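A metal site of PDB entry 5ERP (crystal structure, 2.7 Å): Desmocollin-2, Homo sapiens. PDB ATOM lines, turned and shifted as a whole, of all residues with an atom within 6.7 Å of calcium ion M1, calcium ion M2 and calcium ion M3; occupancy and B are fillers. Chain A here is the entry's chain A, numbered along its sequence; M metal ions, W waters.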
ATOM      1  N   GLU A 247      20.784   6.279  -0.994  1.00  0.00           N
ATOM      2  CA  GLU A 247      22.050   6.073  -1.685  1.00  0.00           C
ATOM      3  C   GLU A 247      23.154   5.596  -0.746  1.00  0.00           C
ATOM      4  O   GLU A 247      24.044   4.856  -1.149  1.00  0.00           O
ATOM      5  CB  GLU A 247      22.473   7.388  -2.354  1.00  0.00           C
ATOM      6  CG  GLU A 247      23.917   7.455  -2.816  1.00  0.00           C
ATOM      7  CD  GLU A 247      24.343   8.861  -3.191  1.00  0.00           C
ATOM      8  OE1 GLU A 247      23.460   9.747  -3.286  1.00  0.00           O
ATOM      9  OE2 GLU A 247      25.553   9.079  -3.378  1.00  0.00           O
ATOM     10  N   LEU A 298      25.797   1.551  -2.634  1.00  0.00           N
ATOM     11  CA  LEU A 298      25.220   2.191  -3.806  1.00  0.00           C
ATOM     12  C   LEU A 298      25.874   3.552  -4.027  1.00  0.00           C
ATOM     13  O   LEU A 298      26.498   4.113  -3.126  1.00  0.00           O
ATOM     14  CB  LEU A 298      23.703   2.344  -3.640  1.00  0.00           C
ATOM     15  CG  LEU A 298      22.969   1.106  -3.110  1.00  0.00           C
ATOM     16  CD1 LEU A 298      21.476   1.373  -2.969  1.00  0.00           C
ATOM     17  CD2 LEU A 298      23.221  -0.107  -3.993  1.00  0.00           C
ATOM     18  N   ASP A 299      25.715   4.084  -5.237  1.00  0.00           N
ATOM     19  CA  ASP A 299      26.236   5.394  -5.595  1.00  0.00           C
ATOM     20  C   ASP A 299      25.354   6.014  -6.662  1.00  0.00           C
ATOM     21  O   ASP A 299      25.357   5.583  -7.812  1.00  0.00           O
ATOM     22  CB  ASP A 299      27.681   5.289  -6.091  1.00  0.00           C
ATOM     23  CG  ASP A 299      28.269   6.635  -6.476  1.00  0.00           C
ATOM     24  OD1 ASP A 299      27.796   7.670  -5.955  1.00  0.00           O
ATOM     25  OD2 ASP A 299      29.186   6.657  -7.315  1.00  0.00           O
ATOM     26  N   ARG A 300      24.584   7.035  -6.284  1.00  0.00           N
ATOM     27  CA  ARG A 300      23.690   7.701  -7.222  1.00  0.00           C
ATOM     28  C   ARG A 300      24.471   8.355  -8.348  1.00  0.00           C
ATOM     29  O   ARG A 300      23.981   8.467  -9.470  1.00  0.00           O
ATOM     30  CB  ARG A 300      22.823   8.737  -6.497  1.00  0.00           C
ATOM     31  CG  ARG A 300      21.914   9.547  -7.408  1.00  0.00           C
ATOM     32  CD  ARG A 300      21.173  10.620  -6.653  1.00  0.00           C
ATOM     33  NE  ARG A 300      20.615  11.641  -7.541  1.00  0.00           N
ATOM     34  CZ  ARG A 300      21.318  12.617  -8.102  1.00  0.00           C
ATOM     35  NH1 ARG A 300      22.623  12.723  -7.876  1.00  0.00           N
ATOM     36  NH2 ARG A 300      20.712  13.492  -8.897  1.00  0.00           N
ATOM     37  N   GLU A 301      25.700   8.761  -8.054  1.00  0.00           N
ATOM     38  CA  GLU A 301      26.494   9.543  -8.998  1.00  0.00           C
ATOM     39  C   GLU A 301      27.442   8.692  -9.843  1.00  0.00           C
ATOM     40  O   GLU A 301      28.265   9.228 -10.577  1.00  0.00           O
ATOM     41  CB  GLU A 301      27.300  10.600  -8.232  1.00  0.00           C
ATOM     42  CG  GLU A 301      26.423  11.591  -7.488  1.00  0.00           C
ATOM     43  CD  GLU A 301      25.908  11.044  -6.173  1.00  0.00           C
ATOM     44  OE1 GLU A 301      26.611  10.212  -5.553  1.00  0.00           O
ATOM     45  OE2 GLU A 301      24.804  11.438  -5.763  1.00  0.00           O
ATOM     46  N   ALA A 302      27.331   7.368  -9.725  1.00  0.00           N
ATOM     47  CA  ALA A 302      28.141   6.463 -10.531  1.00  0.00           C
ATOM     48  C   ALA A 302      27.820   6.643 -12.010  1.00  0.00           C
ATOM     49  O   ALA A 302      26.721   7.104 -12.356  1.00  0.00           O
ATOM     50  CB  ALA A 302      27.921   5.023 -10.107  1.00  0.00           C
ATOM     51  N   GLN A 333      17.767   7.635  -3.671  1.00  0.00           N
ATOM     52  CA  GLN A 333      17.478   8.946  -3.111  1.00  0.00           C
ATOM     53  C   GLN A 333      18.810   9.578  -2.750  1.00  0.00           C
ATOM     54  O   GLN A 333      19.612   8.987  -2.022  1.00  0.00           O
ATOM     55  CB  GLN A 333      16.547   8.841  -1.900  1.00  0.00           C
ATOM     56  CG  GLN A 333      16.087  10.182  -1.360  1.00  0.00           C
ATOM     57  CD  GLN A 333      15.188  10.049  -0.150  1.00  0.00           C
ATOM     58  OE1 GLN A 333      14.723   8.957   0.174  1.00  0.00           O
ATOM     59  NE2 GLN A 333      14.898  11.173   0.495  1.00  0.00           N
ATOM     60  N   ASP A 334      19.053  10.778  -3.262  1.00  0.00           N
ATOM     61  CA  ASP A 334      20.351  11.410  -3.121  1.00  0.00           C
ATOM     62  C   ASP A 334      20.688  11.813  -1.689  1.00  0.00           C
ATOM     63  O   ASP A 334      19.814  12.179  -0.912  1.00  0.00           O
ATOM     64  CB  ASP A 334      20.458  12.649  -4.006  1.00  0.00           C
ATOM     65  CG  ASP A 334      21.835  13.270  -3.978  1.00  0.00           C
ATOM     66  OD1 ASP A 334      22.820  12.547  -4.210  1.00  0.00           O
ATOM     67  OD2 ASP A 334      21.936  14.480  -3.690  1.00  0.00           O
ATOM     68  N   VAL A 335      21.978  11.716  -1.378  1.00  0.00           N
ATOM     69  CA  VAL A 335      22.513  12.180  -0.113  1.00  0.00           C
ATOM     70  C   VAL A 335      23.692  13.094  -0.464  1.00  0.00           C
ATOM     71  O   VAL A 335      24.552  12.713  -1.256  1.00  0.00           O
ATOM     72  CB  VAL A 335      22.992  11.003   0.768  1.00  0.00           C
ATOM     73  CG1 VAL A 335      23.650  11.492   2.042  1.00  0.00           C
ATOM     74  CG2 VAL A 335      21.817  10.074   1.090  1.00  0.00           C
ATOM     75  N   ASN A 336      23.723  14.299   0.107  1.00  0.00           N
ATOM     76  CA  ASN A 336      24.782  15.236  -0.222  1.00  0.00           C
ATOM     77  C   ASN A 336      26.124  14.716   0.285  1.00  0.00           C
ATOM     78  O   ASN A 336      26.550  15.016   1.401  1.00  0.00           O
ATOM     79  CB  ASN A 336      24.506  16.627   0.356  1.00  0.00           C
ATOM     80  CG  ASN A 336      25.375  17.701  -0.279  1.00  0.00           C
ATOM     81  OD1 ASN A 336      26.485  17.434  -0.733  1.00  0.00           O
ATOM     82  ND2 ASN A 336      24.874  18.929  -0.309  1.00  0.00           N
ATOM     83  N   ASP A 337      26.790  13.938  -0.566  1.00  0.00           N
ATOM     84  CA  ASP A 337      28.070  13.319  -0.226  1.00  0.00           C
ATOM     85  C   ASP A 337      29.114  13.637  -1.287  1.00  0.00           C
ATOM     86  O   ASP A 337      30.125  12.940  -1.390  1.00  0.00           O
ATOM     87  CB  ASP A 337      27.907  11.814  -0.066  1.00  0.00           C
ATOM     88  CG  ASP A 337      27.397  11.130  -1.333  1.00  0.00           C
ATOM     89  OD1 ASP A 337      27.094  11.843  -2.317  1.00  0.00           O
ATOM     90  OD2 ASP A 337      27.311   9.882  -1.340  1.00  0.00           O
ATOM     91  N   ASN A 338      28.860  14.671  -2.082  1.00  0.00           N
ATOM     92  CA  ASN A 338      29.790  15.073  -3.126  1.00  0.00           C
ATOM     93  C   ASN A 338      30.041  16.577  -3.151  1.00  0.00           C
ATOM     94  O   ASN A 338      29.116  17.386  -3.064  1.00  0.00           O
ATOM     95  CB  ASN A 338      29.275  14.623  -4.496  1.00  0.00           C
ATOM     96  CG  ASN A 338      29.384  13.122  -4.689  1.00  0.00           C
ATOM     97  OD1 ASN A 338      28.420  12.464  -5.078  1.00  0.00           O
ATOM     98  ND2 ASN A 338      30.548  12.567  -4.404  1.00  0.00           N
ATOM     99  N   SER A 339      31.311  16.938  -3.268  1.00  0.00           N
ATOM    100  CA  SER A 339      31.753  18.321  -3.397  1.00  0.00           C
ATOM    101  C   SER A 339      31.763  18.743  -4.859  1.00  0.00           C
ATOM    102  O   SER A 339      31.685  17.895  -5.749  1.00  0.00           O
ATOM    103  CB  SER A 339      33.145  18.494  -2.785  1.00  0.00           C
ATOM    104  OG  SER A 339      34.006  17.450  -3.207  1.00  0.00           O
ATOM    105  N   PRO A 340      31.844  20.059  -5.118  1.00  0.00           N
ATOM    106  CA  PRO A 340      31.923  20.537  -6.508  1.00  0.00           C
ATOM    107  C   PRO A 340      33.157  20.003  -7.234  1.00  0.00           C
ATOM    108  O   PRO A 340      34.035  19.416  -6.604  1.00  0.00           O
ATOM    109  CB  PRO A 340      32.013  22.066  -6.348  1.00  0.00           C
ATOM    110  CG  PRO A 340      31.416  22.342  -5.008  1.00  0.00           C
ATOM    111  CD  PRO A 340      31.756  21.166  -4.148  1.00  0.00           C
ATOM    112  N   ASP A 363      28.264  20.004  -9.551  1.00  0.00           N
ATOM    113  CA  ASP A 363      28.016  19.165  -8.389  1.00  0.00           C
ATOM    114  C   ASP A 363      27.206  17.938  -8.807  1.00  0.00           C
ATOM    115  O   ASP A 363      26.063  18.071  -9.236  1.00  0.00           O
ATOM    116  CB  ASP A 363      27.287  19.948  -7.298  1.00  0.00           C
ATOM    117  CG  ASP A 363      27.480  19.341  -5.920  1.00  0.00           C
ATOM    118  OD1 ASP A 363      27.417  18.094  -5.800  1.00  0.00           O
ATOM    119  OD2 ASP A 363      27.712  20.105  -4.963  1.00  0.00           O
ATOM    120  N   PRO A 364      27.802  16.731  -8.690  1.00  0.00           N
ATOM    121  CA  PRO A 364      27.118  15.487  -9.088  1.00  0.00           C
ATOM    122  C   PRO A 364      25.775  15.270  -8.392  1.00  0.00           C
ATOM    123  O   PRO A 364      24.894  14.626  -8.950  1.00  0.00           O
ATOM    124  CB  PRO A 364      28.116  14.409  -8.682  1.00  0.00           C
ATOM    125  CG  PRO A 364      29.427  15.064  -8.738  1.00  0.00           C
ATOM    126  CD  PRO A 364      29.187  16.468  -8.266  1.00  0.00           C
ATOM    127  N   ASP A 365      25.632  15.806  -7.175  1.00  0.00           N
ATOM    128  CA  ASP A 365      24.403  15.620  -6.413  1.00  0.00           C
ATOM    129  C   ASP A 365      23.238  16.363  -7.059  1.00  0.00           C
ATOM    130  O   ASP A 365      23.417  17.082  -8.035  1.00  0.00           O
ATOM    131  CB  ASP A 365      24.598  16.107  -4.971  1.00  0.00           C
ATOM    132  CG  ASP A 365      25.697  15.351  -4.242  1.00  0.00           C
ATOM    133  OD1 ASP A 365      25.845  14.135  -4.480  1.00  0.00           O
ATOM    134  OD2 ASP A 365      26.403  15.977  -3.430  1.00  0.00           O
ATOM    135  N   GLU A 366      22.055  16.172  -6.496  1.00  0.00           N
ATOM    136  CA  GLU A 366      20.853  16.822  -7.004  1.00  0.00           C
ATOM    137  C   GLU A 366      20.913  18.333  -6.732  1.00  0.00           C
ATOM    138  O   GLU A 366      21.682  18.770  -5.871  1.00  0.00           O
ATOM    139  CB  GLU A 366      19.613  16.175  -6.374  1.00  0.00           C
ATOM    140  CG  GLU A 366      19.493  16.348  -4.867  1.00  0.00           C
ATOM    141  CD  GLU A 366      18.370  15.523  -4.279  1.00  0.00           C
ATOM    142  OE1 GLU A 366      17.455  15.129  -5.040  1.00  0.00           O
ATOM    143  OE2 GLU A 366      18.398  15.250  -3.059  1.00  0.00           O
ATOM    144  N   HIS A 369      21.276  19.920  -3.449  1.00  0.00           N
ATOM    145  CA  HIS A 369      22.554  19.635  -2.799  1.00  0.00           C
ATOM    146  C   HIS A 369      23.732  20.068  -3.664  1.00  0.00           C
ATOM    147  O   HIS A 369      24.769  19.398  -3.709  1.00  0.00           O
ATOM    148  CB  HIS A 369      22.654  18.147  -2.482  1.00  0.00           C
ATOM    149  CG  HIS A 369      21.688  17.682  -1.441  1.00  0.00           C
ATOM    150  ND1 HIS A 369      21.322  16.366  -1.296  1.00  0.00           N
ATOM    151  CD2 HIS A 369      21.014  18.371  -0.489  1.00  0.00           C
ATOM    152  CE1 HIS A 369      20.455  16.255  -0.297  1.00  0.00           C
ATOM    153  NE2 HIS A 369      20.253  17.453   0.217  1.00  0.00           N
ATOM    154  N   GLY A 370      23.574  21.198  -4.363  1.00  0.00           N
ATOM    155  CA  GLY A 370      24.614  21.711  -5.239  1.00  0.00           C
ATOM    156  C   GLY A 370      24.738  23.227  -5.158  1.00  0.00           C
ATOM    157  O   GLY A 370      25.150  23.753  -4.131  1.00  0.00           O
ATOM    158  N   PHE A 373      27.371  27.950  -5.886  1.00  0.00           N
ATOM    159  CA  PHE A 373      28.735  27.653  -5.470  1.00  0.00           C
ATOM    160  C   PHE A 373      29.472  28.902  -5.023  1.00  0.00           C
ATOM    161  O   PHE A 373      29.252  29.987  -5.561  1.00  0.00           O
ATOM    162  CB  PHE A 373      29.503  26.983  -6.613  1.00  0.00           C
ATOM    163  CG  PHE A 373      28.865  25.732  -7.123  1.00  0.00           C
ATOM    164  CD1 PHE A 373      28.230  24.856  -6.268  1.00  0.00           C
ATOM    165  CD2 PHE A 373      28.903  25.437  -8.480  1.00  0.00           C
ATOM    166  CE1 PHE A 373      27.635  23.697  -6.746  1.00  0.00           C
ATOM    167  CE2 PHE A 373      28.310  24.290  -8.965  1.00  0.00           C
ATOM    168  CZ  PHE A 373      27.682  23.422  -8.095  1.00  0.00           C
ATOM    169  N   ASP A 419      30.014  24.106  -2.076  1.00  0.00           N
ATOM    170  CA  ASP A 419      28.615  24.102  -2.475  1.00  0.00           C
ATOM    171  C   ASP A 419      27.762  24.919  -1.511  1.00  0.00           C
ATOM    172  O   ASP A 419      28.283  25.609  -0.640  1.00  0.00           O
ATOM    173  CB  ASP A 419      28.093  22.667  -2.568  1.00  0.00           C
ATOM    174  CG  ASP A 419      28.157  21.934  -1.238  1.00  0.00           C
ATOM    175  OD1 ASP A 419      28.778  22.456  -0.289  1.00  0.00           O
ATOM    176  OD2 ASP A 419      27.580  20.829  -1.142  1.00  0.00           O
ATOM    177  N   ARG A 420      26.448  24.832  -1.687  1.00  0.00           N
ATOM    178  CA  ARG A 420      25.500  25.564  -0.853  1.00  0.00           C
ATOM    179  C   ARG A 420      25.656  25.235   0.634  1.00  0.00           C
ATOM    180  O   ARG A 420      25.398  26.085   1.481  1.00  0.00           O
ATOM    181  CB  ARG A 420      24.071  25.257  -1.300  1.00  0.00           C
ATOM    182  CG  ARG A 420      23.037  26.249  -0.797  1.00  0.00           C
ATOM    183  CD  ARG A 420      21.648  25.869  -1.282  1.00  0.00           C
ATOM    184  NE  ARG A 420      21.230  24.595  -0.717  1.00  0.00           N
ATOM    185  CZ  ARG A 420      20.661  24.455   0.479  1.00  0.00           C
ATOM    186  NH1 ARG A 420      20.446  25.508   1.249  1.00  0.00           N
ATOM    187  NH2 ARG A 420      20.307  23.249   0.912  1.00  0.00           N
ATOM    188  N   MET A 423      30.336  21.570   1.370  1.00  0.00           N
ATOM    189  CA  MET A 423      31.212  20.502   0.892  1.00  0.00           C
ATOM    190  C   MET A 423      32.240  21.133  -0.037  1.00  0.00           C
ATOM    191  O   MET A 423      31.892  21.624  -1.115  1.00  0.00           O
ATOM    192  CB  MET A 423      30.437  19.403   0.174  1.00  0.00           C
ATOM    193  CG  MET A 423      29.685  18.455   1.098  1.00  0.00           C
ATOM    194  SD  MET A 423      30.800  17.373   2.034  1.00  0.00           S
ATOM    195  CE  MET A 423      31.524  16.378   0.723  1.00  0.00           C
HETATM  196 CA    CA M   1      26.853  18.508  -3.039  1.00  0.00          CA
HETATM  197 CA    CA M   2      25.008  12.003  -3.533  1.00  0.00          CA
HETATM  198 CA    CA M   3      27.928   8.695  -3.749  1.00  0.00          CA
HETATM  199  O   HOH W   1      28.624   6.285  -2.866  1.00  0.00           O
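OD2 of Asp 334 sits at hydrogen-bond distance from N of Glu 366 (3.3 Å).
OD2 of Asp 299 sits at hydrogen-bond distance from N of Ala 302 (3.1 Å).
OE2 of Glu 301 lies close to NH1 of Arg 300 (3.3 Å).
The side-chain amide oxygen (OD1) of Asn 338 lies close to the side-chain carboxylate (OD1) of Asp 337 (3.1 Å).
The side-chain amide nitrogen of Asn 336 is in hydrogen-bond range of the side-chain carboxylate of Asp 419.
The backbone NH (N) of Met 423 sits at hydrogen-bond distance from the side-chain carboxylate (OD1) of Asp 419, at 2.4 Å.
The side-chain carboxylate (OE1) of Glu 301 sits close to the side-chain amide oxygen (OD1) of Asn 338 (2.9 Å).
O of Gln 333 sits at hydrogen-bond distance from N of Glu 247, at 3.1 Å.
Of the 24 residues printed, 6 come within 4 Å of calcium ion M1.
Of the 24 residues printed, 7 come within 4 Å of calcium ion M2.
The nearest printed residue that does not touch calcium ion M2 is Asn 336 (4.5 Å).
Four residues have an atom within 4 Å of calcium ion M3: Glu 247, Asp 299, Glu 301 and Asp 337.
The nearest printed residue that does not touch calcium ion M3 is Asn 338 (4.03 Å).
O of His 369 binds calcium ion M1 (2.4 Å).
O of Asn 338 is bound to calcium ion M1 (2.5 Å).
OD1 of Asn 336 binds calcium ion M1 (2.6 Å).
The side-chain carboxylate (OD2) of Asp 365 binds calcium ion M1, 2.6 Å away.
OD2 of Asp 363 binds calcium ion M1 (2.6 Å).
OD1 of Asp 363 is bound to calcium ion M1 (2.8 Å).
Slightly farther from calcium ion M1 lies the side-chain carboxylate (OD2) of Asp 419 (3.1 Å).
Calcium ion M2 is bound by OE2 of Glu 301, OD1 of Asp 334, OD1 of Asp 337, O of Val 335, OD1 of Asp 365 and OE1 of Glu 247.
Calcium ion M2 has six donor atoms within binding distance.
Slightly farther from calcium ion M2 lies OE2 of Glu 247 (3.0 Å).
Slightly farther from calcium ion M2 lies the side-chain carboxylate (OE1) of Glu 301 (3.1 Å).
Calcium ion M3 is bound by OE2 of Glu 247 (2.4 Å), OD1 of Asp 299 (2.4 Å), water W1 (2.7 Å), OE1 of Glu 301 (2.7 Å) and OD2 of Asp 337 (2.8 Å).
Calcium ion M3 has five donor atoms within binding distance.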
